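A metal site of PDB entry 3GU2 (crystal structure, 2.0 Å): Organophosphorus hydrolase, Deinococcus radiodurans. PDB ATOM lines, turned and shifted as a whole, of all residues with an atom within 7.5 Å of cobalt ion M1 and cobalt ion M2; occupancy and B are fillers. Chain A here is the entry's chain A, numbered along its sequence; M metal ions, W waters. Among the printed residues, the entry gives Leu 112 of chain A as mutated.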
ATOM      1  N   HIS A  36      26.359 -16.538  -6.851  1.00  0.00           N
ATOM      2  CA  HIS A  36      25.915 -16.047  -8.135  1.00  0.00           C
ATOM      3  C   HIS A  36      26.924 -16.385  -9.242  1.00  0.00           C
ATOM      4  O   HIS A  36      27.930 -15.701  -9.416  1.00  0.00           O
ATOM      5  CB  HIS A  36      25.730 -14.531  -8.107  1.00  0.00           C
ATOM      6  CG  HIS A  36      25.056 -13.984  -9.320  1.00  0.00           C
ATOM      7  ND1 HIS A  36      23.901 -13.234  -9.272  1.00  0.00           N
ATOM      8  CD2 HIS A  36      25.374 -14.088 -10.640  1.00  0.00           C
ATOM      9  CE1 HIS A  36      23.534 -12.898 -10.499  1.00  0.00           C
ATOM     10  NE2 HIS A  36      24.413 -13.406 -11.353  1.00  0.00           N
ATOM     11  N   GLU A  37      26.578 -17.396 -10.008  1.00  0.00           N
ATOM     12  CA  GLU A  37      27.438 -17.871 -11.093  1.00  0.00           C
ATOM     13  C   GLU A  37      26.517 -18.437 -12.165  1.00  0.00           C
ATOM     14  O   GLU A  37      25.333 -18.672 -11.927  1.00  0.00           O
ATOM     15  CB  GLU A  37      28.352 -18.981 -10.564  1.00  0.00           C
ATOM     16  CG  GLU A  37      29.237 -18.608  -9.345  1.00  0.00           C
ATOM     17  CD  GLU A  37      30.260 -17.525  -9.661  1.00  0.00           C
ATOM     18  OE1 GLU A  37      30.750 -17.471 -10.810  1.00  0.00           O
ATOM     19  OE2 GLU A  37      30.623 -16.733  -8.763  1.00  0.00           O
ATOM     20  N   HIS A  38      27.056 -18.648 -13.369  1.00  0.00           N
ATOM     21  CA  HIS A  38      26.240 -19.220 -14.443  1.00  0.00           C
ATOM     22  C   HIS A  38      27.031 -20.375 -15.062  1.00  0.00           C
ATOM     23  O   HIS A  38      28.119 -20.169 -15.617  1.00  0.00           O
ATOM     24  CB  HIS A  38      25.939 -18.143 -15.488  1.00  0.00           C
ATOM     25  CG  HIS A  38      25.235 -16.930 -14.951  1.00  0.00           C
ATOM     26  ND1 HIS A  38      23.869 -16.888 -14.758  1.00  0.00           N
ATOM     27  CD2 HIS A  38      25.701 -15.713 -14.562  1.00  0.00           C
ATOM     28  CE1 HIS A  38      23.523 -15.705 -14.283  1.00  0.00           C
ATOM     29  NE2 HIS A  38      24.616 -14.976 -14.159  1.00  0.00           N
ATOM     30  N   PHE A  41      25.164 -19.943 -20.076  1.00  0.00           N
ATOM     31  CA  PHE A  41      24.383 -18.709 -20.161  1.00  0.00           C
ATOM     32  C   PHE A  41      24.313 -18.226 -21.589  1.00  0.00           C
ATOM     33  O   PHE A  41      25.265 -18.352 -22.343  1.00  0.00           O
ATOM     34  CB  PHE A  41      24.985 -17.624 -19.263  1.00  0.00           C
ATOM     35  CG  PHE A  41      24.268 -16.301 -19.338  1.00  0.00           C
ATOM     36  CD1 PHE A  41      24.500 -15.420 -20.385  1.00  0.00           C
ATOM     37  CD2 PHE A  41      23.358 -15.931 -18.349  1.00  0.00           C
ATOM     38  CE1 PHE A  41      23.851 -14.175 -20.452  1.00  0.00           C
ATOM     39  CE2 PHE A  41      22.697 -14.683 -18.408  1.00  0.00           C
ATOM     40  CZ  PHE A  41      22.951 -13.814 -19.459  1.00  0.00           C
ATOM     41  N   ALA A  82      22.538 -18.442 -10.991  1.00  0.00           N
ATOM     42  CA  ALA A  82      21.542 -17.378 -11.107  1.00  0.00           C
ATOM     43  C   ALA A  82      20.928 -17.157 -12.499  1.00  0.00           C
ATOM     44  O   ALA A  82      20.310 -16.109 -12.764  1.00  0.00           O
ATOM     45  CB  ALA A  82      22.160 -16.076 -10.623  1.00  0.00           C
ATOM     46  N   THR A  83      21.100 -18.130 -13.400  1.00  0.00           N
ATOM     47  CA  THR A  83      20.608 -17.982 -14.786  1.00  0.00           C
ATOM     48  C   THR A  83      19.098 -17.881 -14.917  1.00  0.00           C
ATOM     49  O   THR A  83      18.410 -18.841 -14.597  1.00  0.00           O
ATOM     50  CB  THR A  83      21.056 -19.167 -15.680  1.00  0.00           C
ATOM     51  OG1 THR A  83      22.468 -19.386 -15.537  1.00  0.00           O
ATOM     52  CG2 THR A  83      20.743 -18.850 -17.156  1.00  0.00           C
ATOM     53  N   PRO A  84      18.576 -16.751 -15.417  1.00  0.00           N
ATOM     54  CA  PRO A  84      17.128 -16.507 -15.606  1.00  0.00           C
ATOM     55  C   PRO A  84      16.518 -17.448 -16.646  1.00  0.00           C
ATOM     56  O   PRO A  84      17.210 -17.916 -17.560  1.00  0.00           O
ATOM     57  CB  PRO A  84      17.065 -15.045 -16.076  1.00  0.00           C
ATOM     58  CG  PRO A  84      18.354 -14.442 -15.499  1.00  0.00           C
ATOM     59  CD  PRO A  84      19.347 -15.541 -15.740  1.00  0.00           C
ATOM     60  N   LEU A 112      15.021 -11.756 -16.823  1.00  0.00           N
ATOM     61  CA  LEU A 112      15.918 -10.604 -16.871  1.00  0.00           C
ATOM     62  C   LEU A 112      15.064  -9.322 -16.986  1.00  0.00           C
ATOM     63  O   LEU A 112      13.836  -9.405 -17.111  1.00  0.00           O
ATOM     64  CB  LEU A 112      16.852 -10.718 -18.079  1.00  0.00           C
ATOM     65  CG  LEU A 112      18.217 -10.041 -17.957  1.00  0.00           C
ATOM     66  CD1 LEU A 112      18.960 -10.624 -16.772  1.00  0.00           C
ATOM     67  CD2 LEU A 112      19.018 -10.236 -19.249  1.00  0.00           C
ATOM     68  N   TYR A 113      15.691  -8.140 -16.924  1.00  0.00           N
ATOM     69  CA  TYR A 113      14.960  -6.860 -17.029  1.00  0.00           C
ATOM     70  C   TYR A 113      14.284  -6.566 -18.383  1.00  0.00           C
ATOM     71  O   TYR A 113      14.527  -7.256 -19.375  1.00  0.00           O
ATOM     72  CB  TYR A 113      15.865  -5.681 -16.612  1.00  0.00           C
ATOM     73  CG  TYR A 113      17.332  -5.834 -17.010  1.00  0.00           C
ATOM     74  CD1 TYR A 113      18.077  -6.931 -16.568  1.00  0.00           C
ATOM     75  CD2 TYR A 113      17.954  -4.891 -17.827  1.00  0.00           C
ATOM     76  CE1 TYR A 113      19.413  -7.093 -16.934  1.00  0.00           C
ATOM     77  CE2 TYR A 113      19.308  -5.051 -18.205  1.00  0.00           C
ATOM     78  CZ  TYR A 113      20.022  -6.156 -17.755  1.00  0.00           C
ATOM     79  OH  TYR A 113      21.337  -6.336 -18.132  1.00  0.00           O
ATOM     80  N   KCX A 156      15.122 -15.221  -8.842  1.00  0.00           N
ATOM     81  CA  KCX A 156      16.038 -14.229  -9.348  1.00  0.00           C
ATOM     82  CB  KCX A 156      16.837 -14.868 -10.487  1.00  0.00           C
ATOM     83  CG  KCX A 156      17.557 -13.869 -11.370  1.00  0.00           C
ATOM     84  CD  KCX A 156      18.720 -13.258 -10.689  1.00  0.00           C
ATOM     85  CE  KCX A 156      19.905 -13.480 -11.581  1.00  0.00           C
ATOM     86  NZ  KCX A 156      20.506 -12.235 -11.989  1.00  0.00           N
ATOM     87  C   KCX A 156      15.237 -13.024  -9.852  1.00  0.00           C
ATOM     88  O   KCX A 156      14.292 -13.170 -10.616  1.00  0.00           O
ATOM     89  CX  KCX A 156      21.539 -12.151 -12.821  1.00  0.00           C
ATOM     90  OQ1 KCX A 156      22.014 -11.047 -13.113  1.00  0.00           O
ATOM     91  OQ2 KCX A 156      21.954 -13.154 -13.430  1.00  0.00           O
ATOM     92  N   LEU A 157      15.626 -11.840  -9.422  1.00  0.00           N
ATOM     93  CA  LEU A 157      14.958 -10.619  -9.835  1.00  0.00           C
ATOM     94  C   LEU A 157      15.966  -9.664 -10.422  1.00  0.00           C
ATOM     95  O   LEU A 157      17.133  -9.691 -10.041  1.00  0.00           O
ATOM     96  CB  LEU A 157      14.307  -9.946  -8.627  1.00  0.00           C
ATOM     97  CG  LEU A 157      13.179 -10.699  -7.951  1.00  0.00           C
ATOM     98  CD1 LEU A 157      12.601  -9.801  -6.838  1.00  0.00           C
ATOM     99  CD2 LEU A 157      12.103 -11.066  -8.971  1.00  0.00           C
ATOM    100  N   ALA A 158      15.509  -8.794 -11.322  1.00  0.00           N
ATOM    101  CA  ALA A 158      16.380  -7.816 -11.957  1.00  0.00           C
ATOM    102  C   ALA A 158      15.660  -6.478 -12.151  1.00  0.00           C
ATOM    103  O   ALA A 158      14.445  -6.430 -12.337  1.00  0.00           O
ATOM    104  CB  ALA A 158      16.868  -8.351 -13.310  1.00  0.00           C
ATOM    105  N   THR A 188      19.089 -10.812  -6.364  1.00  0.00           N
ATOM    106  CA  THR A 188      18.802  -9.876  -7.430  1.00  0.00           C
ATOM    107  C   THR A 188      19.997  -9.471  -8.279  1.00  0.00           C
ATOM    108  O   THR A 188      21.163  -9.747  -7.965  1.00  0.00           O
ATOM    109  CB  THR A 188      18.242  -8.554  -6.889  1.00  0.00           C
ATOM    110  OG1 THR A 188      19.322  -7.724  -6.440  1.00  0.00           O
ATOM    111  CG2 THR A 188      17.293  -8.823  -5.737  1.00  0.00           C
ATOM    112  N   HIS A 189      19.671  -8.773  -9.348  1.00  0.00           N
ATOM    113  CA  HIS A 189      20.612  -8.186 -10.273  1.00  0.00           C
ATOM    114  C   HIS A 189      20.311  -6.694 -10.164  1.00  0.00           C
ATOM    115  O   HIS A 189      19.133  -6.308 -10.140  1.00  0.00           O
ATOM    116  CB  HIS A 189      20.307  -8.682 -11.707  1.00  0.00           C
ATOM    117  CG  HIS A 189      20.735  -7.733 -12.791  1.00  0.00           C
ATOM    118  ND1 HIS A 189      21.843  -7.934 -13.576  1.00  0.00           N
ATOM    119  CD2 HIS A 189      20.187  -6.558 -13.232  1.00  0.00           C
ATOM    120  CE1 HIS A 189      21.973  -6.952 -14.456  1.00  0.00           C
ATOM    121  NE2 HIS A 189      20.974  -6.100 -14.266  1.00  0.00           N
ATOM    122  N   THR A 190      21.338  -5.852 -10.045  1.00  0.00           N
ATOM    123  CA  THR A 190      21.108  -4.410 -10.065  1.00  0.00           C
ATOM    124  C   THR A 190      21.906  -3.950 -11.279  1.00  0.00           C
ATOM    125  O   THR A 190      22.982  -4.491 -11.562  1.00  0.00           O
ATOM    126  CB  THR A 190      21.638  -3.657  -8.809  1.00  0.00           C
ATOM    127  OG1 THR A 190      23.020  -3.967  -8.603  1.00  0.00           O
ATOM    128  CG2 THR A 190      20.822  -4.032  -7.563  1.00  0.00           C
ATOM    129  N   GLN A 191      21.382  -2.977 -12.000  1.00  0.00           N
ATOM    130  CA  GLN A 191      22.029  -2.474 -13.213  1.00  0.00           C
ATOM    131  C   GLN A 191      22.934  -1.290 -12.944  1.00  0.00           C
ATOM    132  O   GLN A 191      22.489  -0.257 -12.410  1.00  0.00           O
ATOM    133  CB  GLN A 191      20.971  -2.066 -14.236  1.00  0.00           C
ATOM    134  CG  GLN A 191      21.522  -1.750 -15.630  1.00  0.00           C
ATOM    135  CD  GLN A 191      22.179  -2.961 -16.280  1.00  0.00           C
ATOM    136  OE1 GLN A 191      21.801  -4.114 -16.037  1.00  0.00           O
ATOM    137  NE2 GLN A 191      23.171  -2.697 -17.130  1.00  0.00           N
ATOM    138  N   GLY A 216      21.975  -8.179  -5.443  1.00  0.00           N
ATOM    139  CA  GLY A 216      23.191  -8.401  -6.220  1.00  0.00           C
ATOM    140  C   GLY A 216      23.868  -7.238  -6.924  1.00  0.00           C
ATOM    141  O   GLY A 216      23.393  -6.094  -6.915  1.00  0.00           O
ATOM    142  N   HIS A 217      24.998  -7.543  -7.560  1.00  0.00           N
ATOM    143  CA  HIS A 217      25.811  -6.589  -8.291  1.00  0.00           C
ATOM    144  C   HIS A 217      26.027  -5.274  -7.568  1.00  0.00           C
ATOM    145  O   HIS A 217      26.097  -4.215  -8.201  1.00  0.00           O
ATOM    146  CB  HIS A 217      25.223  -6.299  -9.671  1.00  0.00           C
ATOM    147  CG  HIS A 217      24.923  -7.529 -10.463  1.00  0.00           C
ATOM    148  ND1 HIS A 217      25.564  -8.728 -10.239  1.00  0.00           N
ATOM    149  CD2 HIS A 217      23.997  -7.785 -11.422  1.00  0.00           C
ATOM    150  CE1 HIS A 217      25.045  -9.662 -10.999  1.00  0.00           C
ATOM    151  NE2 HIS A 217      24.093  -9.112 -11.729  1.00  0.00           N
ATOM    152  N   ASP A 240      29.106  -9.647  -6.315  1.00  0.00           N
ATOM    153  CA  ASP A 240      29.071 -10.849  -7.110  1.00  0.00           C
ATOM    154  C   ASP A 240      29.592 -10.776  -8.563  1.00  0.00           C
ATOM    155  O   ASP A 240      29.290 -11.646  -9.375  1.00  0.00           O
ATOM    156  CB  ASP A 240      27.639 -11.417  -7.089  1.00  0.00           C
ATOM    157  CG  ASP A 240      26.592 -10.394  -7.554  1.00  0.00           C
ATOM    158  OD1 ASP A 240      26.939  -9.566  -8.404  1.00  0.00           O
ATOM    159  OD2 ASP A 240      25.424 -10.431  -7.090  1.00  0.00           O
ATOM    160  N   ARG A 241      30.384  -9.763  -8.879  1.00  0.00           N
ATOM    161  CA  ARG A 241      30.927  -9.674 -10.235  1.00  0.00           C
ATOM    162  C   ARG A 241      32.423  -9.414 -10.141  1.00  0.00           C
ATOM    163  O   ARG A 241      33.018  -8.704 -10.957  1.00  0.00           O
ATOM    164  CB  ARG A 241      30.223  -8.562 -11.014  1.00  0.00           C
ATOM    165  CG  ARG A 241      28.723  -8.749 -11.087  1.00  0.00           C
ATOM    166  CD  ARG A 241      28.066  -7.848 -12.124  1.00  0.00           C
ATOM    167  NE  ARG A 241      28.470  -8.237 -13.467  1.00  0.00           N
ATOM    168  CZ  ARG A 241      27.951  -7.750 -14.586  1.00  0.00           C
ATOM    169  NH1 ARG A 241      26.984  -6.847 -14.526  1.00  0.00           N
ATOM    170  NH2 ARG A 241      28.411  -8.161 -15.761  1.00  0.00           N
ATOM    171  N   HIS A 276      31.468 -14.173  -8.604  1.00  0.00           N
ATOM    172  CA  HIS A 276      32.075 -13.663  -9.825  1.00  0.00           C
ATOM    173  C   HIS A 276      31.083 -13.308 -10.924  1.00  0.00           C
ATOM    174  O   HIS A 276      31.327 -12.378 -11.717  1.00  0.00           O
ATOM    175  CB  HIS A 276      33.061 -14.695 -10.414  1.00  0.00           C
ATOM    176  CG  HIS A 276      33.982 -15.323  -9.409  1.00  0.00           C
ATOM    177  ND1 HIS A 276      33.661 -16.467  -8.713  1.00  0.00           N
ATOM    178  CD2 HIS A 276      35.241 -14.992  -9.017  1.00  0.00           C
ATOM    179  CE1 HIS A 276      34.669 -16.816  -7.934  1.00  0.00           C
ATOM    180  NE2 HIS A 276      35.642 -15.937  -8.095  1.00  0.00           N
ATOM    181  N   ASP A 277      29.993 -14.055 -10.977  1.00  0.00           N
ATOM    182  CA  ASP A 277      28.990 -13.883 -12.033  1.00  0.00           C
ATOM    183  C   ASP A 277      29.632 -14.352 -13.355  1.00  0.00           C
ATOM    184  O   ASP A 277      29.407 -13.774 -14.418  1.00  0.00           O
ATOM    185  CB  ASP A 277      28.551 -12.429 -12.160  1.00  0.00           C
ATOM    186  CG  ASP A 277      27.435 -12.268 -13.160  1.00  0.00           C
ATOM    187  OD1 ASP A 277      26.708 -13.259 -13.357  1.00  0.00           O
ATOM    188  OD2 ASP A 277      27.280 -11.184 -13.730  1.00  0.00           O
ATOM    189  N   SER A 278      30.403 -15.424 -13.263  1.00  0.00           N
ATOM    190  CA  SER A 278      31.090 -15.971 -14.413  1.00  0.00           C
ATOM    191  C   SER A 278      30.181 -16.850 -15.260  1.00  0.00           C
ATOM    192  O   SER A 278      29.097 -17.244 -14.822  1.00  0.00           O
ATOM    193  CB  SER A 278      32.294 -16.792 -13.922  1.00  0.00           C
ATOM    194  OG  SER A 278      31.854 -17.887 -13.149  1.00  0.00           O
ATOM    195  N   ILE A 279      30.649 -17.156 -16.469  1.00  0.00           N
ATOM    196  CA  ILE A 279      29.907 -18.020 -17.373  1.00  0.00           C
ATOM    197  C   ILE A 279      30.870 -19.115 -17.765  1.00  0.00           C
ATOM    198  O   ILE A 279      31.898 -18.851 -18.383  1.00  0.00           O
ATOM    199  CB  ILE A 279      29.455 -17.236 -18.615  1.00  0.00           C
ATOM    200  CG1 ILE A 279      28.412 -16.189 -18.182  1.00  0.00           C
ATOM    201  CG2 ILE A 279      28.896 -18.210 -19.683  1.00  0.00           C
ATOM    202  CD1 ILE A 279      28.011 -15.209 -19.236  1.00  0.00           C
HETATM  203 CO    CO M   1      23.196  -9.824 -13.718  1.00  0.00          CO
HETATM  204 CO    CO M   2      24.418 -13.026 -13.546  1.00  0.00          CO
HETATM  205  O   HOH W   1      24.769  -8.211 -14.745  1.00  0.00           O
HETATM  206  O   HOH W   2      22.607 -10.247 -15.917  1.00  0.00           O
HETATM  207  O   HOH W   3      25.691 -11.221 -15.589  1.00  0.00           O
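The backbone NH of His 189 lies within hydrogen-bond range of the backbone carbonyl oxygen of Leu 157 (2.8 Å).
OD2 of Asp 277 lies within salt-bridge range of NE of Arg 241, at 3.2 Å.
ND1 of His 217 lies within hydrogen-bond range of OD1 of Asp 240 (2.4 Å).
OG1 of Thr 83 lies within hydrogen-bond range of ND1 of His 38, 3.0 Å away.
The backbone NH (N) of Asp 277 sits at hydrogen-bond distance from the backbone carbonyl oxygen (O) of Asp 240, 3.0 Å away.
The side-chain amide oxygen of Gln 191 is in hydrogen-bond range of a ring nitrogen (NE2) of His 189.
The backbone carbonyl oxygen (O) of His 217 sits at hydrogen-bond distance from the side-chain hydroxyl (OG1) of Thr 190, 3.1 Å away.
The backbone NH (N) of His 38 is in hydrogen-bond range of the backbone carbonyl oxygen (O) of Ser 278 (2.9 Å).
Cobalt ion M2 is bound by a ring nitrogen (NE2) of His 38 (2.1 Å), a ring nitrogen (NE2) of His 36 (2.2 Å), the side-chain carboxylate (OD1) of Asp 277 (2.3 Å) and OQ2 of KCX 156 (2.5 Å).
Cobalt ion M2 has four donor atoms within binding distance.
Cobalt ion M1 is bound by OQ1 of KCX 156 (1.8 Å), a ring nitrogen (NE2) of His 217 (2.3 Å), water W2 (2.3 Å), a ring nitrogen (ND1) of His 189 (2.3 Å) and water W1 (2.5 Å).
Cobalt ion M1 has five donor atoms within binding distance.
Within 4 Å of cobalt ion M2: His 36, His 38, KCX 156 and Asp 277.
Three residues have an atom within 4 Å of cobalt ion M1: KCX 156, His 189 and His 217.
The nearest printed residue that does not touch cobalt ion M1 is Asp 277 (4.3 Å).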
